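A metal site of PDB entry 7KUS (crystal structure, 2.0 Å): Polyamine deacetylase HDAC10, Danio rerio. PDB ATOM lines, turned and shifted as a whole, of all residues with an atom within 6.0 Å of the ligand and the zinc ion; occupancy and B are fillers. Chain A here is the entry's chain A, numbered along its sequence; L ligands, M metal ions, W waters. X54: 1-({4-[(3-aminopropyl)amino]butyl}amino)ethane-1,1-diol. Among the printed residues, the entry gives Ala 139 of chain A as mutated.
Of the 25 residues printed, 3 come within 4 Å of the zinc ion.
The nearest printed residue that does not touch the zinc ion is Val 177 (4.1 Å).
N05 of the ligand sits close to OH of Tyr 309, 3.5 Å away.
O03 of the ligand lies within hydrogen-bond range of NE2 of His 138.
OE2 of Glu 26 is in salt-bridge range of N10 of the ligand, 3.4 Å away.
N05 of the ligand sits at hydrogen-bond distance from O of Gly 147 (3.2 Å).
Water W2 lies within hydrogen-bond range of the backbone carbonyl oxygen (O) of Glu 26, a nitrogen (N10) of the ligand and the side-chain carboxylate (OE1) of Glu 276.
Water W1 bridges OE2 of Glu 276 and N10 of the ligand.
The side-chain carboxylate of Asp 176 lies within hydrogen-bond range of the backbone NH of Gly 307, at 3.0 Å.
OD1 of Asp 269 lies within hydrogen-bond range of N of Val 177, 2.8 Å away.
A ring nitrogen (NE2) of His 178 is in hydrogen-bond range of the side-chain carboxylate of Glu 276 (2.8 Å).
The backbone NH (N) of His 138 sits at hydrogen-bond distance from the side-chain sulfur (SG) of Cys 149.
The backbone NH (N) of His 138 sits at hydrogen-bond distance from the side-chain carboxylate (OE1) of Glu 306 (2.9 Å).
O of Gly 147 lies within hydrogen-bond range of SG of Cys 149 (3.4 Å).
The backbone NH of Gly 147 sits at hydrogen-bond distance from the backbone carbonyl oxygen of Asn 95 (2.9 Å).
O of Ala 96 sits at hydrogen-bond distance from N of Phe 148, 2.8 Å away.
Ala 96 touches the ligand (CB to C09, 3.7 Å).
Pro 136 touches the ligand (CG to C01, 3.96 Å).
Phe 148 touches the ligand.
CD2 of Trp 207 touches C09 of the ligand, 3.7 Å away.
Glu 276 touches the ligand.
Gly 307 touches the ligand (N to C01, 3.9 Å).
Within 4 Å of the ligand: Glu 26, Ala 96, Pro 136, His 138, Gly 147, Phe 148, Asp 176, His 178, Trp 207, Asp 269, Glu 276, Gly 307 and Tyr 309.
The zinc ion is bound by OD2 of Asp 176, O04 of the ligand, OD2 of Asp 269 and ND1 of His 178.
Slightly farther from the zinc ion lies O03 of the ligand (2.6 Å).
Slightly farther from the zinc ion lies the side-chain carboxylate (OD1) of Asp 176 (2.7 Å).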
ATOM      1  N   PRO A  25     -23.569 -30.448  -3.094  1.00  0.00           N
ATOM      2  CA  PRO A  25     -22.695 -31.576  -3.484  1.00  0.00           C
ATOM      3  C   PRO A  25     -21.922 -31.318  -4.766  1.00  0.00           C
ATOM      4  O   PRO A  25     -20.811 -31.833  -4.931  1.00  0.00           O
ATOM      5  CB  PRO A  25     -23.683 -32.746  -3.648  1.00  0.00           C
ATOM      6  CG  PRO A  25     -24.951 -32.303  -2.980  1.00  0.00           C
ATOM      7  CD  PRO A  25     -24.994 -30.805  -3.091  1.00  0.00           C
ATOM      8  N   GLU A  26     -22.479 -30.493  -5.655  1.00  0.00           N
ATOM      9  CA  GLU A  26     -21.807 -30.205  -6.921  1.00  0.00           C
ATOM     10  C   GLU A  26     -20.496 -29.438  -6.698  1.00  0.00           C
ATOM     11  O   GLU A  26     -19.485 -29.739  -7.351  1.00  0.00           O
ATOM     12  CB  GLU A  26     -22.768 -29.428  -7.817  1.00  0.00           C
ATOM     13  CG  GLU A  26     -22.177 -29.035  -9.147  1.00  0.00           C
ATOM     14  CD  GLU A  26     -23.226 -28.534 -10.122  1.00  0.00           C
ATOM     15  OE1 GLU A  26     -24.208 -27.915  -9.670  1.00  0.00           O
ATOM     16  OE2 GLU A  26     -23.075 -28.761 -11.335  1.00  0.00           O
ATOM     17  N   CYS A  27     -20.495 -28.467  -5.788  1.00  0.00           N
ATOM     18  CA  CYS A  27     -19.329 -27.620  -5.579  1.00  0.00           C
ATOM     19  C   CYS A  27     -18.448 -28.027  -4.407  1.00  0.00           C
ATOM     20  O   CYS A  27     -17.343 -27.486  -4.271  1.00  0.00           O
ATOM     21  CB  CYS A  27     -19.755 -26.153  -5.377  1.00  0.00           C
ATOM     22  SG  CYS A  27     -20.595 -25.409  -6.791  1.00  0.00           S
ATOM     23  N   ILE A  29     -16.454 -30.265  -3.860  1.00  0.00           N
ATOM     24  CA  ILE A  29     -15.125 -30.800  -4.169  1.00  0.00           C
ATOM     25  C   ILE A  29     -14.073 -29.707  -4.329  1.00  0.00           C
ATOM     26  O   ILE A  29     -12.868 -29.994  -4.284  1.00  0.00           O
ATOM     27  CB  ILE A  29     -15.148 -31.629  -5.460  1.00  0.00           C
ATOM     28  CG1 ILE A  29     -15.693 -30.776  -6.603  1.00  0.00           C
ATOM     29  CG2 ILE A  29     -15.987 -32.892  -5.279  1.00  0.00           C
ATOM     30  CD1 ILE A  29     -15.505 -31.408  -7.990  1.00  0.00           C
ATOM     31  N   ASN A  95     -23.950 -21.227 -13.169  1.00  0.00           N
ATOM     32  CA  ASN A  95     -23.851 -22.683 -13.261  1.00  0.00           C
ATOM     33  C   ASN A  95     -22.636 -23.176 -12.484  1.00  0.00           C
ATOM     34  O   ASN A  95     -21.501 -22.837 -12.829  1.00  0.00           O
ATOM     35  CB  ASN A  95     -23.764 -23.067 -14.743  1.00  0.00           C
ATOM     36  CG  ASN A  95     -23.781 -24.554 -14.998  1.00  0.00           C
ATOM     37  OD1 ASN A  95     -23.766 -25.377 -14.080  1.00  0.00           O
ATOM     38  ND2 ASN A  95     -23.813 -24.920 -16.277  1.00  0.00           N
ATOM     39  N   ALA A  96     -22.877 -23.977 -11.428  1.00  0.00           N
ATOM     40  CA  ALA A  96     -21.815 -24.695 -10.714  1.00  0.00           C
ATOM     41  C   ALA A  96     -20.714 -23.750 -10.187  1.00  0.00           C
ATOM     42  O   ALA A  96     -19.533 -23.930 -10.470  1.00  0.00           O
ATOM     43  CB  ALA A  96     -21.213 -25.787 -11.603  1.00  0.00           C
ATOM     44  N   PRO A 136     -10.006 -21.428 -10.032  1.00  0.00           N
ATOM     45  CA  PRO A 136      -9.593 -21.724 -11.401  1.00  0.00           C
ATOM     46  C   PRO A 136     -10.309 -20.783 -12.366  1.00  0.00           C
ATOM     47  O   PRO A 136     -11.166 -19.984 -11.980  1.00  0.00           O
ATOM     48  CB  PRO A 136     -10.015 -23.178 -11.615  1.00  0.00           C
ATOM     49  CG  PRO A 136     -11.178 -23.372 -10.686  1.00  0.00           C
ATOM     50  CD  PRO A 136     -10.908 -22.464  -9.479  1.00  0.00           C
ATOM     51  N   GLY A 137      -9.933 -20.866 -13.638  1.00  0.00           N
ATOM     52  CA  GLY A 137     -10.430 -19.879 -14.566  1.00  0.00           C
ATOM     53  C   GLY A 137     -11.102 -20.326 -15.848  1.00  0.00           C
ATOM     54  O   GLY A 137     -11.960 -19.585 -16.346  1.00  0.00           O
ATOM     55  N   HIS A 138     -10.794 -21.517 -16.385  1.00  0.00           N
ATOM     56  CA  HIS A 138     -11.024 -21.760 -17.821  1.00  0.00           C
ATOM     57  C   HIS A 138     -12.498 -21.874 -18.206  1.00  0.00           C
ATOM     58  O   HIS A 138     -12.812 -21.756 -19.395  1.00  0.00           O
ATOM     59  CB  HIS A 138     -10.228 -22.998 -18.301  1.00  0.00           C
ATOM     60  CG  HIS A 138     -10.772 -24.311 -17.831  1.00  0.00           C
ATOM     61  ND1 HIS A 138     -10.593 -25.487 -18.544  1.00  0.00           N
ATOM     62  CD2 HIS A 138     -11.443 -24.666 -16.703  1.00  0.00           C
ATOM     63  CE1 HIS A 138     -11.136 -26.488 -17.887  1.00  0.00           C
ATOM     64  NE2 HIS A 138     -11.659 -26.021 -16.768  1.00  0.00           N
ATOM     65  N   ALA A 139     -13.401 -22.074 -17.262  1.00  0.00           N
ATOM     66  CA  ALA A 139     -14.827 -22.099 -17.576  1.00  0.00           C
ATOM     67  C   ALA A 139     -15.475 -20.727 -17.459  1.00  0.00           C
ATOM     68  O   ALA A 139     -16.631 -20.578 -17.860  1.00  0.00           O
ATOM     69  CB  ALA A 139     -15.566 -23.077 -16.663  1.00  0.00           C
ATOM     70  N   GLY A 147     -18.661 -22.980 -13.293  1.00  0.00           N
ATOM     71  CA  GLY A 147     -17.818 -24.134 -13.032  1.00  0.00           C
ATOM     72  C   GLY A 147     -16.642 -23.848 -12.116  1.00  0.00           C
ATOM     73  O   GLY A 147     -15.508 -24.159 -12.455  1.00  0.00           O
ATOM     74  N   PHE A 148     -16.914 -23.236 -10.965  1.00  0.00           N
ATOM     75  CA  PHE A 148     -15.938 -22.848  -9.944  1.00  0.00           C
ATOM     76  C   PHE A 148     -15.057 -21.690 -10.374  1.00  0.00           C
ATOM     77  O   PHE A 148     -14.159 -21.299  -9.607  1.00  0.00           O
ATOM     78  CB  PHE A 148     -14.997 -24.000  -9.508  1.00  0.00           C
ATOM     79  CG  PHE A 148     -15.685 -25.331  -9.275  1.00  0.00           C
ATOM     80  CD1 PHE A 148     -17.008 -25.396  -8.861  1.00  0.00           C
ATOM     81  CD2 PHE A 148     -14.977 -26.520  -9.439  1.00  0.00           C
ATOM     82  CE1 PHE A 148     -17.617 -26.627  -8.629  1.00  0.00           C
ATOM     83  CE2 PHE A 148     -15.585 -27.748  -9.198  1.00  0.00           C
ATOM     84  CZ  PHE A 148     -16.902 -27.790  -8.803  1.00  0.00           C
ATOM     85  N   CYS A 149     -15.241 -21.140 -11.560  1.00  0.00           N
ATOM     86  CA  CYS A 149     -14.369 -20.105 -12.098  1.00  0.00           C
ATOM     87  C   CYS A 149     -15.035 -18.734 -12.042  1.00  0.00           C
ATOM     88  O   CYS A 149     -16.202 -18.578 -12.432  1.00  0.00           O
ATOM     89  CB  CYS A 149     -13.962 -20.431 -13.531  1.00  0.00           C
ATOM     90  SG  CYS A 149     -13.208 -22.074 -13.759  1.00  0.00           S
ATOM     91  N   ASP A 176      -6.915 -30.065 -18.400  1.00  0.00           N
ATOM     92  CA  ASP A 176      -8.005 -30.287 -17.462  1.00  0.00           C
ATOM     93  C   ASP A 176      -9.005 -31.248 -18.095  1.00  0.00           C
ATOM     94  O   ASP A 176      -9.137 -31.296 -19.322  1.00  0.00           O
ATOM     95  CB  ASP A 176      -8.658 -28.938 -17.135  1.00  0.00           C
ATOM     96  CG  ASP A 176      -9.651 -29.010 -15.984  1.00  0.00           C
ATOM     97  OD1 ASP A 176      -9.311 -28.596 -14.863  1.00  0.00           O
ATOM     98  OD2 ASP A 176     -10.786 -29.498 -16.174  1.00  0.00           O
ATOM     99  N   VAL A 177      -9.702 -32.023 -17.253  1.00  0.00           N
ATOM    100  CA  VAL A 177     -10.628 -33.023 -17.779  1.00  0.00           C
ATOM    101  C   VAL A 177     -11.954 -32.420 -18.224  1.00  0.00           C
ATOM    102  O   VAL A 177     -12.760 -33.112 -18.856  1.00  0.00           O
ATOM    103  CB  VAL A 177     -10.877 -34.137 -16.749  1.00  0.00           C
ATOM    104  CG1 VAL A 177     -12.005 -33.742 -15.769  1.00  0.00           C
ATOM    105  CG2 VAL A 177     -11.184 -35.470 -17.454  1.00  0.00           C
ATOM    106  N   HIS A 178     -12.218 -31.152 -17.910  1.00  0.00           N
ATOM    107  CA  HIS A 178     -13.388 -30.436 -18.383  1.00  0.00           C
ATOM    108  C   HIS A 178     -13.003 -29.546 -19.543  1.00  0.00           C
ATOM    109  O   HIS A 178     -11.861 -29.063 -19.638  1.00  0.00           O
ATOM    110  CB  HIS A 178     -14.013 -29.580 -17.256  1.00  0.00           C
ATOM    111  CG  HIS A 178     -14.436 -30.366 -16.060  1.00  0.00           C
ATOM    112  ND1 HIS A 178     -13.611 -30.592 -14.979  1.00  0.00           N
ATOM    113  CD2 HIS A 178     -15.610 -30.994 -15.765  1.00  0.00           C
ATOM    114  CE1 HIS A 178     -14.252 -31.298 -14.072  1.00  0.00           C
ATOM    115  NE2 HIS A 178     -15.467 -31.565 -14.522  1.00  0.00           N
ATOM    116  N   HIS A 179     -13.955 -29.321 -20.434  1.00  0.00           N
ATOM    117  CA  HIS A 179     -13.754 -28.348 -21.507  1.00  0.00           C
ATOM    118  C   HIS A 179     -13.604 -26.952 -20.915  1.00  0.00           C
ATOM    119  O   HIS A 179     -14.303 -26.587 -19.969  1.00  0.00           O
ATOM    120  CB  HIS A 179     -14.954 -28.366 -22.463  1.00  0.00           C
ATOM    121  CG  HIS A 179     -14.737 -27.589 -23.710  1.00  0.00           C
ATOM    122  ND1 HIS A 179     -15.724 -26.839 -24.318  1.00  0.00           N
ATOM    123  CD2 HIS A 179     -13.624 -27.414 -24.456  1.00  0.00           C
ATOM    124  CE1 HIS A 179     -15.223 -26.262 -25.395  1.00  0.00           C
ATOM    125  NE2 HIS A 179     -13.960 -26.599 -25.502  1.00  0.00           N
ATOM    126  N   TRP A 207     -20.808 -32.646 -17.963  1.00  0.00           N
ATOM    127  CA  TRP A 207     -20.683 -31.205 -17.763  1.00  0.00           C
ATOM    128  C   TRP A 207     -19.504 -30.645 -18.557  1.00  0.00           C
ATOM    129  O   TRP A 207     -18.414 -31.231 -18.527  1.00  0.00           O
ATOM    130  CB  TRP A 207     -20.519 -30.923 -16.255  1.00  0.00           C
ATOM    131  CG  TRP A 207     -20.690 -29.489 -15.944  1.00  0.00           C
ATOM    132  CD1 TRP A 207     -21.831 -28.874 -15.531  1.00  0.00           C
ATOM    133  CD2 TRP A 207     -19.690 -28.470 -16.051  1.00  0.00           C
ATOM    134  NE1 TRP A 207     -21.609 -27.518 -15.372  1.00  0.00           N
ATOM    135  CE2 TRP A 207     -20.304 -27.254 -15.687  1.00  0.00           C
ATOM    136  CE3 TRP A 207     -18.346 -28.458 -16.441  1.00  0.00           C
ATOM    137  CZ2 TRP A 207     -19.606 -26.035 -15.684  1.00  0.00           C
ATOM    138  CZ3 TRP A 207     -17.655 -27.241 -16.426  1.00  0.00           C
ATOM    139  CH2 TRP A 207     -18.292 -26.048 -16.062  1.00  0.00           C
ATOM    140  N   GLY A 267      -5.336 -28.679 -15.424  1.00  0.00           N
ATOM    141  CA  GLY A 267      -6.246 -29.319 -14.508  1.00  0.00           C
ATOM    142  C   GLY A 267      -5.817 -30.759 -14.358  1.00  0.00           C
ATOM    143  O   GLY A 267      -5.650 -31.484 -15.351  1.00  0.00           O
ATOM    144  N   ASP A 269      -7.591 -32.909 -12.669  1.00  0.00           N
ATOM    145  CA  ASP A 269      -8.725 -33.813 -12.599  1.00  0.00           C
ATOM    146  C   ASP A 269      -8.731 -34.809 -13.755  1.00  0.00           C
ATOM    147  O   ASP A 269      -9.647 -35.642 -13.837  1.00  0.00           O
ATOM    148  CB  ASP A 269     -10.059 -33.058 -12.530  1.00  0.00           C
ATOM    149  CG  ASP A 269     -10.176 -31.927 -13.530  1.00  0.00           C
ATOM    150  OD1 ASP A 269      -9.385 -31.862 -14.489  1.00  0.00           O
ATOM    151  OD2 ASP A 269     -11.116 -31.104 -13.342  1.00  0.00           O
ATOM    152  N   GLU A 276     -14.247 -36.243 -10.544  1.00  0.00           N
ATOM    153  CA  GLU A 276     -14.883 -35.658 -11.725  1.00  0.00           C
ATOM    154  C   GLU A 276     -14.465 -36.350 -13.011  1.00  0.00           C
ATOM    155  O   GLU A 276     -15.307 -36.629 -13.876  1.00  0.00           O
ATOM    156  CB  GLU A 276     -14.547 -34.171 -11.816  1.00  0.00           C
ATOM    157  CG  GLU A 276     -15.362 -33.297 -10.910  1.00  0.00           C
ATOM    158  CD  GLU A 276     -16.803 -33.190 -11.370  1.00  0.00           C
ATOM    159  OE1 GLU A 276     -17.691 -33.546 -10.580  1.00  0.00           O
ATOM    160  OE2 GLU A 276     -17.044 -32.745 -12.526  1.00  0.00           O
ATOM    161  N   GLU A 306      -5.688 -25.334 -12.852  1.00  0.00           N
ATOM    162  CA  GLU A 306      -7.140 -25.242 -12.956  1.00  0.00           C
ATOM    163  C   GLU A 306      -7.808 -26.157 -11.936  1.00  0.00           C
ATOM    164  O   GLU A 306      -7.797 -25.844 -10.733  1.00  0.00           O
ATOM    165  CB  GLU A 306      -7.606 -25.589 -14.386  1.00  0.00           C
ATOM    166  CG  GLU A 306      -6.973 -24.687 -15.429  1.00  0.00           C
ATOM    167  CD  GLU A 306      -7.749 -23.362 -15.658  1.00  0.00           C
ATOM    168  OE1 GLU A 306      -8.760 -23.111 -14.968  1.00  0.00           O
ATOM    169  OE2 GLU A 306      -7.360 -22.583 -16.560  1.00  0.00           O
ATOM    170  N   GLY A 307      -8.371 -27.289 -12.380  1.00  0.00           N
ATOM    171  CA  GLY A 307      -9.001 -28.248 -11.490  1.00  0.00           C
ATOM    172  C   GLY A 307      -8.044 -29.318 -10.987  1.00  0.00           C
ATOM    173  O   GLY A 307      -6.836 -29.267 -11.199  1.00  0.00           O
ATOM    174  N   GLY A 308      -8.619 -30.312 -10.274  1.00  0.00           N
ATOM    175  CA  GLY A 308      -7.877 -31.398  -9.638  1.00  0.00           C
ATOM    176  C   GLY A 308      -8.383 -31.654  -8.227  1.00  0.00           C
ATOM    177  O   GLY A 308      -8.137 -30.843  -7.325  1.00  0.00           O
ATOM    178  N   TYR A 309      -9.163 -32.726  -8.010  1.00  0.00           N
ATOM    179  CA  TYR A 309      -9.982 -32.796  -6.812  1.00  0.00           C
ATOM    180  C   TYR A 309      -9.698 -33.973  -5.897  1.00  0.00           C
ATOM    181  O   TYR A 309     -10.226 -34.010  -4.786  1.00  0.00           O
ATOM    182  CB  TYR A 309     -11.475 -32.792  -7.189  1.00  0.00           C
ATOM    183  CG  TYR A 309     -11.764 -31.611  -8.074  1.00  0.00           C
ATOM    184  CD1 TYR A 309     -11.846 -30.344  -7.542  1.00  0.00           C
ATOM    185  CD2 TYR A 309     -11.869 -31.758  -9.443  1.00  0.00           C
ATOM    186  CE1 TYR A 309     -12.068 -29.245  -8.336  1.00  0.00           C
ATOM    187  CE2 TYR A 309     -12.096 -30.668 -10.265  1.00  0.00           C
ATOM    188  CZ  TYR A 309     -12.188 -29.412  -9.707  1.00  0.00           C
ATOM    189  OH  TYR A 309     -12.393 -28.329 -10.509  1.00  0.00           O
HETATM  190  C13 X54 L   1     -21.130 -32.751 -10.805  1.00  0.00           C
HETATM  191  C01 X54 L   1     -12.112 -26.315 -13.168  1.00  0.00           C
HETATM  192  C02 X54 L   1     -13.107 -27.401 -13.603  1.00  0.00           C
HETATM  193  C06 X54 L   1     -15.370 -28.213 -13.103  1.00  0.00           C
HETATM  194  C07 X54 L   1     -16.795 -27.826 -12.658  1.00  0.00           C
HETATM  195  C08 X54 L   1     -17.674 -29.058 -12.449  1.00  0.00           C
HETATM  196  C09 X54 L   1     -19.183 -28.783 -12.380  1.00  0.00           C
HETATM  197  C11 X54 L   1     -20.831 -30.559 -12.261  1.00  0.00           C
HETATM  198  C12 X54 L   1     -21.737 -31.468 -11.408  1.00  0.00           C
HETATM  199  N05 X54 L   1     -14.429 -27.098 -13.062  1.00  0.00           N
HETATM  200  N10 X54 L   1     -19.851 -29.760 -11.531  1.00  0.00           N
HETATM  201  N14 X54 L   1     -21.970 -33.271  -9.737  1.00  0.00           N
HETATM  202  O03 X54 L   1     -13.110 -27.417 -14.997  1.00  0.00           O
HETATM  203  O04 X54 L   1     -12.593 -28.607 -13.148  1.00  0.00           O
HETATM  204 ZN    ZN M   1     -11.762 -29.651 -14.565  1.00  0.00          ZN
HETATM  205  O   HOH W   1     -19.149 -32.277 -13.816  1.00  0.00           O
HETATM  206  O   HOH W   2     -18.985 -31.141  -9.473  1.00  0.00           O
HETATM  207  O   HOH W   3     -19.477 -35.322 -11.670  1.00  0.00           O
